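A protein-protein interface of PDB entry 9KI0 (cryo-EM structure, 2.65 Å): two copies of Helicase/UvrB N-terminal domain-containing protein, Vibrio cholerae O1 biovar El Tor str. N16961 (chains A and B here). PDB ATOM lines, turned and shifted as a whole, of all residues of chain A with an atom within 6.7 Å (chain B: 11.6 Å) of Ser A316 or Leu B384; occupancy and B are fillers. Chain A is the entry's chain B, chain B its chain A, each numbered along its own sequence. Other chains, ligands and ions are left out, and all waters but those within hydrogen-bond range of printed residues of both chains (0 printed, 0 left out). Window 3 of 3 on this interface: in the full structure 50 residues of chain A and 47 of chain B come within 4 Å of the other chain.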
ATOM      1  N   LEU A 314      12.063  25.009  17.967  1.00  0.00           N
ATOM      2  CA  LEU A 314      11.705  23.603  18.022  1.00  0.00           C
ATOM      3  C   LEU A 314      10.241  23.420  17.639  1.00  0.00           C
ATOM      4  O   LEU A 314       9.440  24.356  17.678  1.00  0.00           O
ATOM      5  CB  LEU A 314      11.936  23.036  19.423  1.00  0.00           C
ATOM      6  CG  LEU A 314      13.358  22.714  19.862  1.00  0.00           C
ATOM      7  CD1 LEU A 314      13.405  22.625  21.369  1.00  0.00           C
ATOM      8  CD2 LEU A 314      13.833  21.418  19.243  1.00  0.00           C
ATOM      9  N   GLU A 315       9.897  22.192  17.271  1.00  0.00           N
ATOM     10  CA  GLU A 315       8.512  21.879  16.963  1.00  0.00           C
ATOM     11  C   GLU A 315       7.673  21.916  18.236  1.00  0.00           C
ATOM     12  O   GLU A 315       8.144  21.582  19.326  1.00  0.00           O
ATOM     13  CB  GLU A 315       8.417  20.507  16.292  1.00  0.00           C
ATOM     14  CG  GLU A 315       7.014  19.939  16.199  1.00  0.00           C
ATOM     15  CD  GLU A 315       6.929  18.737  15.288  1.00  0.00           C
ATOM     16  OE1 GLU A 315       7.959  18.056  15.100  1.00  0.00           O
ATOM     17  OE2 GLU A 315       5.831  18.469  14.760  1.00  0.00           O
ATOM     18  N   SER A 316       6.418  22.343  18.094  1.00  0.00           N
ATOM     19  CA  SER A 316       5.465  22.307  19.203  1.00  0.00           C
ATOM     20  C   SER A 316       4.810  20.930  19.222  1.00  0.00           C
ATOM     21  O   SER A 316       3.691  20.723  18.749  1.00  0.00           O
ATOM     22  CB  SER A 316       4.439  23.424  19.070  1.00  0.00           C
ATOM     23  OG  SER A 316       4.888  24.605  19.710  1.00  0.00           O
ATOM     24  N   SER A 317       5.536  19.974  19.786  1.00  0.00           N
ATOM     25  CA  SER A 317       5.130  18.582  19.861  1.00  0.00           C
ATOM     26  C   SER A 317       5.245  18.096  21.297  1.00  0.00           C
ATOM     27  O   SER A 317       6.026  18.644  22.079  1.00  0.00           O
ATOM     28  CB  SER A 317       6.000  17.707  18.948  1.00  0.00           C
ATOM     29  OG  SER A 317       5.357  16.487  18.629  1.00  0.00           O
ATOM     30  N   PRO A 318       4.468  17.079  21.677  1.00  0.00           N
ATOM     31  CA  PRO A 318       4.663  16.474  23.004  1.00  0.00           C
ATOM     32  C   PRO A 318       6.047  15.881  23.190  1.00  0.00           C
ATOM     33  O   PRO A 318       6.503  15.754  24.331  1.00  0.00           O
ATOM     34  CB  PRO A 318       3.577  15.388  23.071  1.00  0.00           C
ATOM     35  CG  PRO A 318       3.002  15.287  21.697  1.00  0.00           C
ATOM     36  CD  PRO A 318       3.256  16.582  21.010  1.00  0.00           C
ATOM     37  N   ARG A 319       6.723  15.508  22.103  1.00  0.00           N
ATOM     38  CA  ARG A 319       8.082  14.990  22.205  1.00  0.00           C
ATOM     39  C   ARG A 319       9.050  16.057  22.699  1.00  0.00           C
ATOM     40  O   ARG A 319       9.979  15.756  23.457  1.00  0.00           O
ATOM     41  CB  ARG A 319       8.517  14.435  20.850  1.00  0.00           C
ATOM     42  CG  ARG A 319      10.008  14.298  20.670  1.00  0.00           C
ATOM     43  CD  ARG A 319      10.358  13.895  19.249  1.00  0.00           C
ATOM     44  NE  ARG A 319       9.229  13.288  18.557  1.00  0.00           N
ATOM     45  CZ  ARG A 319       9.075  11.983  18.378  1.00  0.00           C
ATOM     46  NH1 ARG A 319       9.964  11.114  18.830  1.00  0.00           N
ATOM     47  NH2 ARG A 319       8.003  11.540  17.730  1.00  0.00           N
ATOM     48  N   TYR A 320       8.847  17.309  22.290  1.00  0.00           N
ATOM     49  CA  TYR A 320       9.706  18.417  22.683  1.00  0.00           C
ATOM     50  C   TYR A 320       9.101  19.244  23.809  1.00  0.00           C
ATOM     51  O   TYR A 320       9.399  20.434  23.936  1.00  0.00           O
ATOM     52  CB  TYR A 320      10.012  19.299  21.476  1.00  0.00           C
ATOM     53  CG  TYR A 320      10.701  18.545  20.372  1.00  0.00           C
ATOM     54  CD1 TYR A 320      12.045  18.225  20.460  1.00  0.00           C
ATOM     55  CD2 TYR A 320      10.001  18.130  19.252  1.00  0.00           C
ATOM     56  CE1 TYR A 320      12.676  17.529  19.460  1.00  0.00           C
ATOM     57  CE2 TYR A 320      10.622  17.432  18.248  1.00  0.00           C
ATOM     58  CZ  TYR A 320      11.959  17.133  18.356  1.00  0.00           C
ATOM     59  OH  TYR A 320      12.586  16.433  17.354  1.00  0.00           O
ATOM     60  N   GLU A 324      11.924  23.780  25.110  1.00  0.00           N
ATOM     61  CA  GLU A 324      12.143  25.132  24.604  1.00  0.00           C
ATOM     62  C   GLU A 324      12.363  26.136  25.730  1.00  0.00           C
ATOM     63  O   GLU A 324      13.036  27.152  25.525  1.00  0.00           O
ATOM     64  CB  GLU A 324      10.961  25.557  23.733  1.00  0.00           C
ATOM     65  CG  GLU A 324      11.182  26.846  22.955  1.00  0.00           C
ATOM     66  CD  GLU A 324      11.597  26.601  21.515  1.00  0.00           C
ATOM     67  OE1 GLU A 324      10.705  26.451  20.655  1.00  0.00           O
ATOM     68  OE2 GLU A 324      12.815  26.564  21.244  1.00  0.00           O
ATOM     69  N   ASN B 342       9.514  30.551   5.408  1.00  0.00           N
ATOM     70  CA  ASN B 342       9.475  30.315   6.852  1.00  0.00           C
ATOM     71  C   ASN B 342      10.615  29.390   7.292  1.00  0.00           C
ATOM     72  O   ASN B 342      10.413  28.270   7.757  1.00  0.00           O
ATOM     73  CB  ASN B 342       8.115  29.745   7.273  1.00  0.00           C
ATOM     74  CG  ASN B 342       7.030  30.794   7.305  1.00  0.00           C
ATOM     75  OD1 ASN B 342       7.091  31.742   8.086  1.00  0.00           O
ATOM     76  ND2 ASN B 342       6.027  30.634   6.452  1.00  0.00           N
ATOM     77  N   ALA B 344      12.563  29.754   9.753  1.00  0.00           N
ATOM     78  CA  ALA B 344      12.714  29.594  11.194  1.00  0.00           C
ATOM     79  C   ALA B 344      12.359  28.185  11.650  1.00  0.00           C
ATOM     80  O   ALA B 344      12.858  27.729  12.683  1.00  0.00           O
ATOM     81  CB  ALA B 344      11.853  30.618  11.928  1.00  0.00           C
ATOM     82  N   PHE B 345      11.511  27.485  10.905  1.00  0.00           N
ATOM     83  CA  PHE B 345      11.097  26.134  11.245  1.00  0.00           C
ATOM     84  C   PHE B 345      11.899  25.109  10.452  1.00  0.00           C
ATOM     85  O   PHE B 345      12.520  25.423   9.434  1.00  0.00           O
ATOM     86  CB  PHE B 345       9.605  25.928  10.972  1.00  0.00           C
ATOM     87  CG  PHE B 345       8.722  27.014  11.511  1.00  0.00           C
ATOM     88  CD1 PHE B 345       9.010  27.637  12.711  1.00  0.00           C
ATOM     89  CD2 PHE B 345       7.588  27.400  10.820  1.00  0.00           C
ATOM     90  CE1 PHE B 345       8.191  28.631  13.203  1.00  0.00           C
ATOM     91  CE2 PHE B 345       6.765  28.390  11.307  1.00  0.00           C
ATOM     92  CZ  PHE B 345       7.068  29.008  12.500  1.00  0.00           C
ATOM     93  N   ALA B 346      11.871  23.870  10.929  1.00  0.00           N
ATOM     94  CA  ALA B 346      12.486  22.755  10.231  1.00  0.00           C
ATOM     95  C   ALA B 346      11.422  22.034   9.409  1.00  0.00           C
ATOM     96  O   ALA B 346      10.234  22.350   9.481  1.00  0.00           O
ATOM     97  CB  ALA B 346      13.171  21.812  11.223  1.00  0.00           C
ATOM     98  N   PHE B 347      11.851  21.028   8.650  1.00  0.00           N
ATOM     99  CA  PHE B 347      11.018  20.378   7.648  1.00  0.00           C
ATOM    100  C   PHE B 347      10.781  18.919   8.008  1.00  0.00           C
ATOM    101  O   PHE B 347      11.677  18.242   8.514  1.00  0.00           O
ATOM    102  CB  PHE B 347      11.662  20.457   6.258  1.00  0.00           C
ATOM    103  CG  PHE B 347      11.734  21.847   5.696  1.00  0.00           C
ATOM    104  CD1 PHE B 347      12.693  22.739   6.141  1.00  0.00           C
ATOM    105  CD2 PHE B 347      10.852  22.258   4.716  1.00  0.00           C
ATOM    106  CE1 PHE B 347      12.761  24.016   5.629  1.00  0.00           C
ATOM    107  CE2 PHE B 347      10.918  23.534   4.199  1.00  0.00           C
ATOM    108  CZ  PHE B 347      11.873  24.413   4.656  1.00  0.00           C
ATOM    109  N   ASN B 348       9.569  18.443   7.734  1.00  0.00           N
ATOM    110  CA  ASN B 348       9.224  17.040   7.902  1.00  0.00           C
ATOM    111  C   ASN B 348       8.134  16.680   6.907  1.00  0.00           C
ATOM    112  O   ASN B 348       7.444  17.549   6.374  1.00  0.00           O
ATOM    113  CB  ASN B 348       8.764  16.737   9.332  1.00  0.00           C
ATOM    114  CG  ASN B 348       8.714  15.252   9.626  1.00  0.00           C
ATOM    115  OD1 ASN B 348       9.386  14.456   8.974  1.00  0.00           O
ATOM    116  ND2 ASN B 348       7.906  14.872  10.606  1.00  0.00           N
ATOM    117  N   GLU B 350       4.737  13.929   5.865  1.00  0.00           N
ATOM    118  CA  GLU B 350       3.567  13.332   6.496  1.00  0.00           C
ATOM    119  C   GLU B 350       2.721  12.661   5.426  1.00  0.00           C
ATOM    120  O   GLU B 350       2.666  13.121   4.281  1.00  0.00           O
ATOM    121  CB  GLU B 350       2.736  14.371   7.262  1.00  0.00           C
ATOM    122  CG  GLU B 350       1.764  15.160   6.412  1.00  0.00           C
ATOM    123  CD  GLU B 350       1.268  16.404   7.112  1.00  0.00           C
ATOM    124  OE1 GLU B 350       2.100  17.122   7.701  1.00  0.00           O
ATOM    125  OE2 GLU B 350       0.047  16.663   7.076  1.00  0.00           O
ATOM    126  N   LYS B 380       3.694  23.264   3.272  1.00  0.00           N
ATOM    127  CA  LYS B 380       2.832  24.131   4.062  1.00  0.00           C
ATOM    128  C   LYS B 380       3.484  24.418   5.405  1.00  0.00           C
ATOM    129  O   LYS B 380       4.146  23.553   5.977  1.00  0.00           O
ATOM    130  CB  LYS B 380       1.451  23.484   4.252  1.00  0.00           C
ATOM    131  CG  LYS B 380       0.902  23.529   5.664  1.00  0.00           C
ATOM    132  CD  LYS B 380      -0.330  22.651   5.796  1.00  0.00           C
ATOM    133  CE  LYS B 380       0.041  21.178   5.785  1.00  0.00           C
ATOM    134  NZ  LYS B 380      -1.128  20.301   6.065  1.00  0.00           N
ATOM    135  N   SER B 381       3.296  25.630   5.913  1.00  0.00           N
ATOM    136  CA  SER B 381       3.840  26.004   7.211  1.00  0.00           C
ATOM    137  C   SER B 381       2.746  25.933   8.267  1.00  0.00           C
ATOM    138  O   SER B 381       1.690  26.558   8.121  1.00  0.00           O
ATOM    139  CB  SER B 381       4.435  27.410   7.165  1.00  0.00           C
ATOM    140  OG  SER B 381       5.674  27.417   6.480  1.00  0.00           O
ATOM    141  N   ASP B 382       3.002  25.168   9.325  1.00  0.00           N
ATOM    142  CA  ASP B 382       2.090  25.022  10.451  1.00  0.00           C
ATOM    143  C   ASP B 382       2.664  25.843  11.598  1.00  0.00           C
ATOM    144  O   ASP B 382       3.662  25.454  12.221  1.00  0.00           O
ATOM    145  CB  ASP B 382       1.920  23.555  10.829  1.00  0.00           C
ATOM    146  CG  ASP B 382       0.595  23.279  11.510  1.00  0.00           C
ATOM    147  OD1 ASP B 382      -0.043  24.241  11.985  1.00  0.00           O
ATOM    148  OD2 ASP B 382       0.189  22.099  11.568  1.00  0.00           O
ATOM    149  N   PHE B 383       2.054  27.009  11.835  1.00  0.00           N
ATOM    150  CA  PHE B 383       2.518  27.941  12.851  1.00  0.00           C
ATOM    151  C   PHE B 383       2.148  27.494  14.256  1.00  0.00           C
ATOM    152  O   PHE B 383       2.792  27.920  15.219  1.00  0.00           O
ATOM    153  CB  PHE B 383       1.946  29.333  12.584  1.00  0.00           C
ATOM    154  CG  PHE B 383       2.632  30.064  11.470  1.00  0.00           C
ATOM    155  CD1 PHE B 383       2.266  29.846  10.155  1.00  0.00           C
ATOM    156  CD2 PHE B 383       3.646  30.968  11.737  1.00  0.00           C
ATOM    157  CE1 PHE B 383       2.896  30.515   9.126  1.00  0.00           C
ATOM    158  CE2 PHE B 383       4.279  31.641  10.711  1.00  0.00           C
ATOM    159  CZ  PHE B 383       3.903  31.413   9.404  1.00  0.00           C
ATOM    160  N   LEU B 384       1.120  26.652  14.393  1.00  0.00           N
ATOM    161  CA  LEU B 384       0.812  26.082  15.698  1.00  0.00           C
ATOM    162  C   LEU B 384       1.823  25.005  16.058  1.00  0.00           C
ATOM    163  O   LEU B 384       2.265  24.916  17.209  1.00  0.00           O
ATOM    164  CB  LEU B 384      -0.608  25.517  15.709  1.00  0.00           C
ATOM    165  CG  LEU B 384      -1.711  26.454  16.200  1.00  0.00           C
ATOM    166  CD1 LEU B 384      -1.345  27.042  17.554  1.00  0.00           C
ATOM    167  CD2 LEU B 384      -1.982  27.555  15.186  1.00  0.00           C
ATOM    168  N   ARG B 385       2.200  24.183  15.083  1.00  0.00           N
ATOM    169  CA  ARG B 385       3.172  23.124  15.284  1.00  0.00           C
ATOM    170  C   ARG B 385       4.598  23.611  15.103  1.00  0.00           C
ATOM    171  O   ARG B 385       5.529  22.904  15.503  1.00  0.00           O
ATOM    172  CB  ARG B 385       2.917  21.967  14.315  1.00  0.00           C
ATOM    173  CG  ARG B 385       1.916  20.942  14.801  1.00  0.00           C
ATOM    174  CD  ARG B 385       1.601  19.954  13.697  1.00  0.00           C
ATOM    175  NE  ARG B 385       2.739  19.083  13.430  1.00  0.00           N
ATOM    176  CZ  ARG B 385       2.698  18.006  12.658  1.00  0.00           C
ATOM    177  NH1 ARG B 385       1.585  17.639  12.044  1.00  0.00           N
ATOM    178  NH2 ARG B 385       3.800  17.280  12.498  1.00  0.00           N
ATOM    179  N   ARG B 386       4.784  24.796  14.514  1.00  0.00           N
ATOM    180  CA  ARG B 386       6.108  25.320  14.188  1.00  0.00           C
ATOM    181  C   ARG B 386       6.878  24.331  13.317  1.00  0.00           C
ATOM    182  O   ARG B 386       8.030  23.991  13.595  1.00  0.00           O
ATOM    183  CB  ARG B 386       6.891  25.664  15.456  1.00  0.00           C
ATOM    184  CG  ARG B 386       6.429  26.927  16.149  1.00  0.00           C
ATOM    185  CD  ARG B 386       6.467  26.759  17.654  1.00  0.00           C
ATOM    186  NE  ARG B 386       6.682  28.023  18.345  1.00  0.00           N
ATOM    187  CZ  ARG B 386       7.538  28.192  19.344  1.00  0.00           C
ATOM    188  NH1 ARG B 386       8.281  27.194  19.793  1.00  0.00           N
ATOM    189  NH2 ARG B 386       7.653  29.394  19.902  1.00  0.00           N
ATOM    190  N   LYS B 387       6.228  23.851  12.257  1.00  0.00           N
ATOM    191  CA  LYS B 387       6.889  22.922  11.349  1.00  0.00           C
ATOM    192  C   LYS B 387       6.536  23.233   9.902  1.00  0.00           C
ATOM    193  O   LYS B 387       5.464  23.759   9.608  1.00  0.00           O
ATOM    194  CB  LYS B 387       6.499  21.472  11.668  1.00  0.00           C
ATOM    195  CG  LYS B 387       7.584  20.652  12.339  1.00  0.00           C
ATOM    196  CD  LYS B 387       8.724  20.354  11.394  1.00  0.00           C
ATOM    197  CE  LYS B 387       9.881  19.702  12.120  1.00  0.00           C
ATOM    198  NZ  LYS B 387       9.464  18.461  12.813  1.00  0.00           N
ATOM    199  N   ASN B 388       7.446  22.895   8.991  1.00  0.00           N
ATOM    200  CA  ASN B 388       7.174  22.934   7.563  1.00  0.00           C
ATOM    201  C   ASN B 388       6.909  21.509   7.095  1.00  0.00           C
ATOM    202  O   ASN B 388       7.796  20.655   7.166  1.00  0.00           O
ATOM    203  CB  ASN B 388       8.351  23.543   6.804  1.00  0.00           C
ATOM    204  CG  ASN B 388       8.459  25.037   7.001  1.00  0.00           C
ATOM    205  OD1 ASN B 388       7.455  25.742   7.042  1.00  0.00           O
ATOM    206  ND2 ASN B 388       9.683  25.527   7.130  1.00  0.00           N
ATOM    207  N   LEU B 389       5.711  21.268   6.578  1.00  0.00           N
ATOM    208  CA  LEU B 389       5.226  19.931   6.284  1.00  0.00           C
ATOM    209  C   LEU B 389       5.150  19.725   4.779  1.00  0.00           C
ATOM    210  O   LEU B 389       4.615  20.573   4.054  1.00  0.00           O
ATOM    211  CB  LEU B 389       3.857  19.704   6.923  1.00  0.00           C
ATOM    212  CG  LEU B 389       3.806  20.043   8.412  1.00  0.00           C
ATOM    213  CD1 LEU B 389       2.373  20.211   8.876  1.00  0.00           C
ATOM    214  CD2 LEU B 389       4.517  18.977   9.223  1.00  0.00           C
ATOM    215  N   ASP B 517      11.841  12.889  12.785  1.00  0.00           N
ATOM    216  CA  ASP B 517      10.896  13.984  12.608  1.00  0.00           C
ATOM    217  C   ASP B 517      11.465  15.153  11.812  1.00  0.00           C
ATOM    218  O   ASP B 517      10.858  16.230  11.813  1.00  0.00           O
ATOM    219  CB  ASP B 517      10.399  14.484  13.967  1.00  0.00           C
ATOM    220  CG  ASP B 517      11.495  15.132  14.783  1.00  0.00           C
ATOM    221  OD1 ASP B 517      12.678  14.781  14.592  1.00  0.00           O
ATOM    222  OD2 ASP B 517      11.172  15.998  15.618  1.00  0.00           O
ATOM    223  N   THR B 518      12.604  14.986  11.148  1.00  0.00           N
ATOM    224  CA  THR B 518      13.118  15.994  10.234  1.00  0.00           C
ATOM    225  C   THR B 518      13.594  15.311   8.964  1.00  0.00           C
ATOM    226  O   THR B 518      14.024  14.156   8.987  1.00  0.00           O
ATOM    227  CB  THR B 518      14.274  16.804  10.836  1.00  0.00           C
ATOM    228  OG1 THR B 518      15.294  15.913  11.300  1.00  0.00           O
ATOM    229  CG2 THR B 518      13.795  17.673  11.985  1.00  0.00           C
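The side-chain amide nitrogen (ND2) of Asn B348 lies close to the backbone carbonyl oxygen (O) of Asp B517, 3.5 Å away. The backbone carbonyl oxygen (O) of Lys B387 lies within hydrogen-bond range of the backbone NH (N) of Asp B382 (2.9 Å). O of Asp B517 is in hydrogen-bond range of NZ of Lys B387 (2.8 Å). The backbone NH (N) of Leu A314 is in hydrogen-bond range of the side-chain carboxylate (OE1) of Glu A324 (3.3 Å).
No position is printed for both chains.
Among the printed residues, merely in contact across the chains: Leu A314 with Arg B386 (3.6 Å), Glu A315 with Asp B517 (3.9 Å), Ser A316 with Leu B384 (3.2 Å) and Ser A316 with Arg B386 (3.4 Å).
Of the 19 printed residues of chain B, 5 touch a printed residue of chain A. Of the 8 printed residues of chain A, 5 touch a printed residue of chain B. Printed residues of chain A that touch a printed residue of chain B: Leu A314, Glu A315, Ser A316, Tyr A320 and Glu A324. Among the printed residues, 9 pairs touch across the chains.
The side-chain carboxylate (OE2) of Glu A315 is in salt-bridge range of the guanidinium group (NH2) of Arg B385 (3.3 Å). The backbone carbonyl oxygen (O) of Arg B385 lies within hydrogen-bond range of the backbone NH (N) of Ser A316 (2.8 Å). OE1 of Glu A324 lies within salt-bridge range of NH1 of Arg B386. The side-chain amino group (NZ) of Lys B387 lies within salt-bridge range of the side-chain carboxylate (OE1) of Glu A315 (2.8 Å). OD1 of Asp B517 lies close to OH of Tyr A320 (3.2 Å).
Ser A316 touches three residues of chain B. No residue of chain B comes within 4 Å of Ser A317. Phe B347 touches none of the printed residues of chain A. Phe B383 touches none of the printed residues of chain A. Of chain A, only Ser A316 comes within 4 Å of Leu B384. Of the printed residues of chain A, Arg B386 touches Leu A314, Ser A316 and Glu A324. Of the printed residues of chain A, Lys B387 touches Glu A315. Printed residues of chain A within 4 Å of Asp B517: Glu A315 and Tyr A320. The nearest residue of chain B that does not touch Ser A316 is Phe B383 (6.0 Å).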
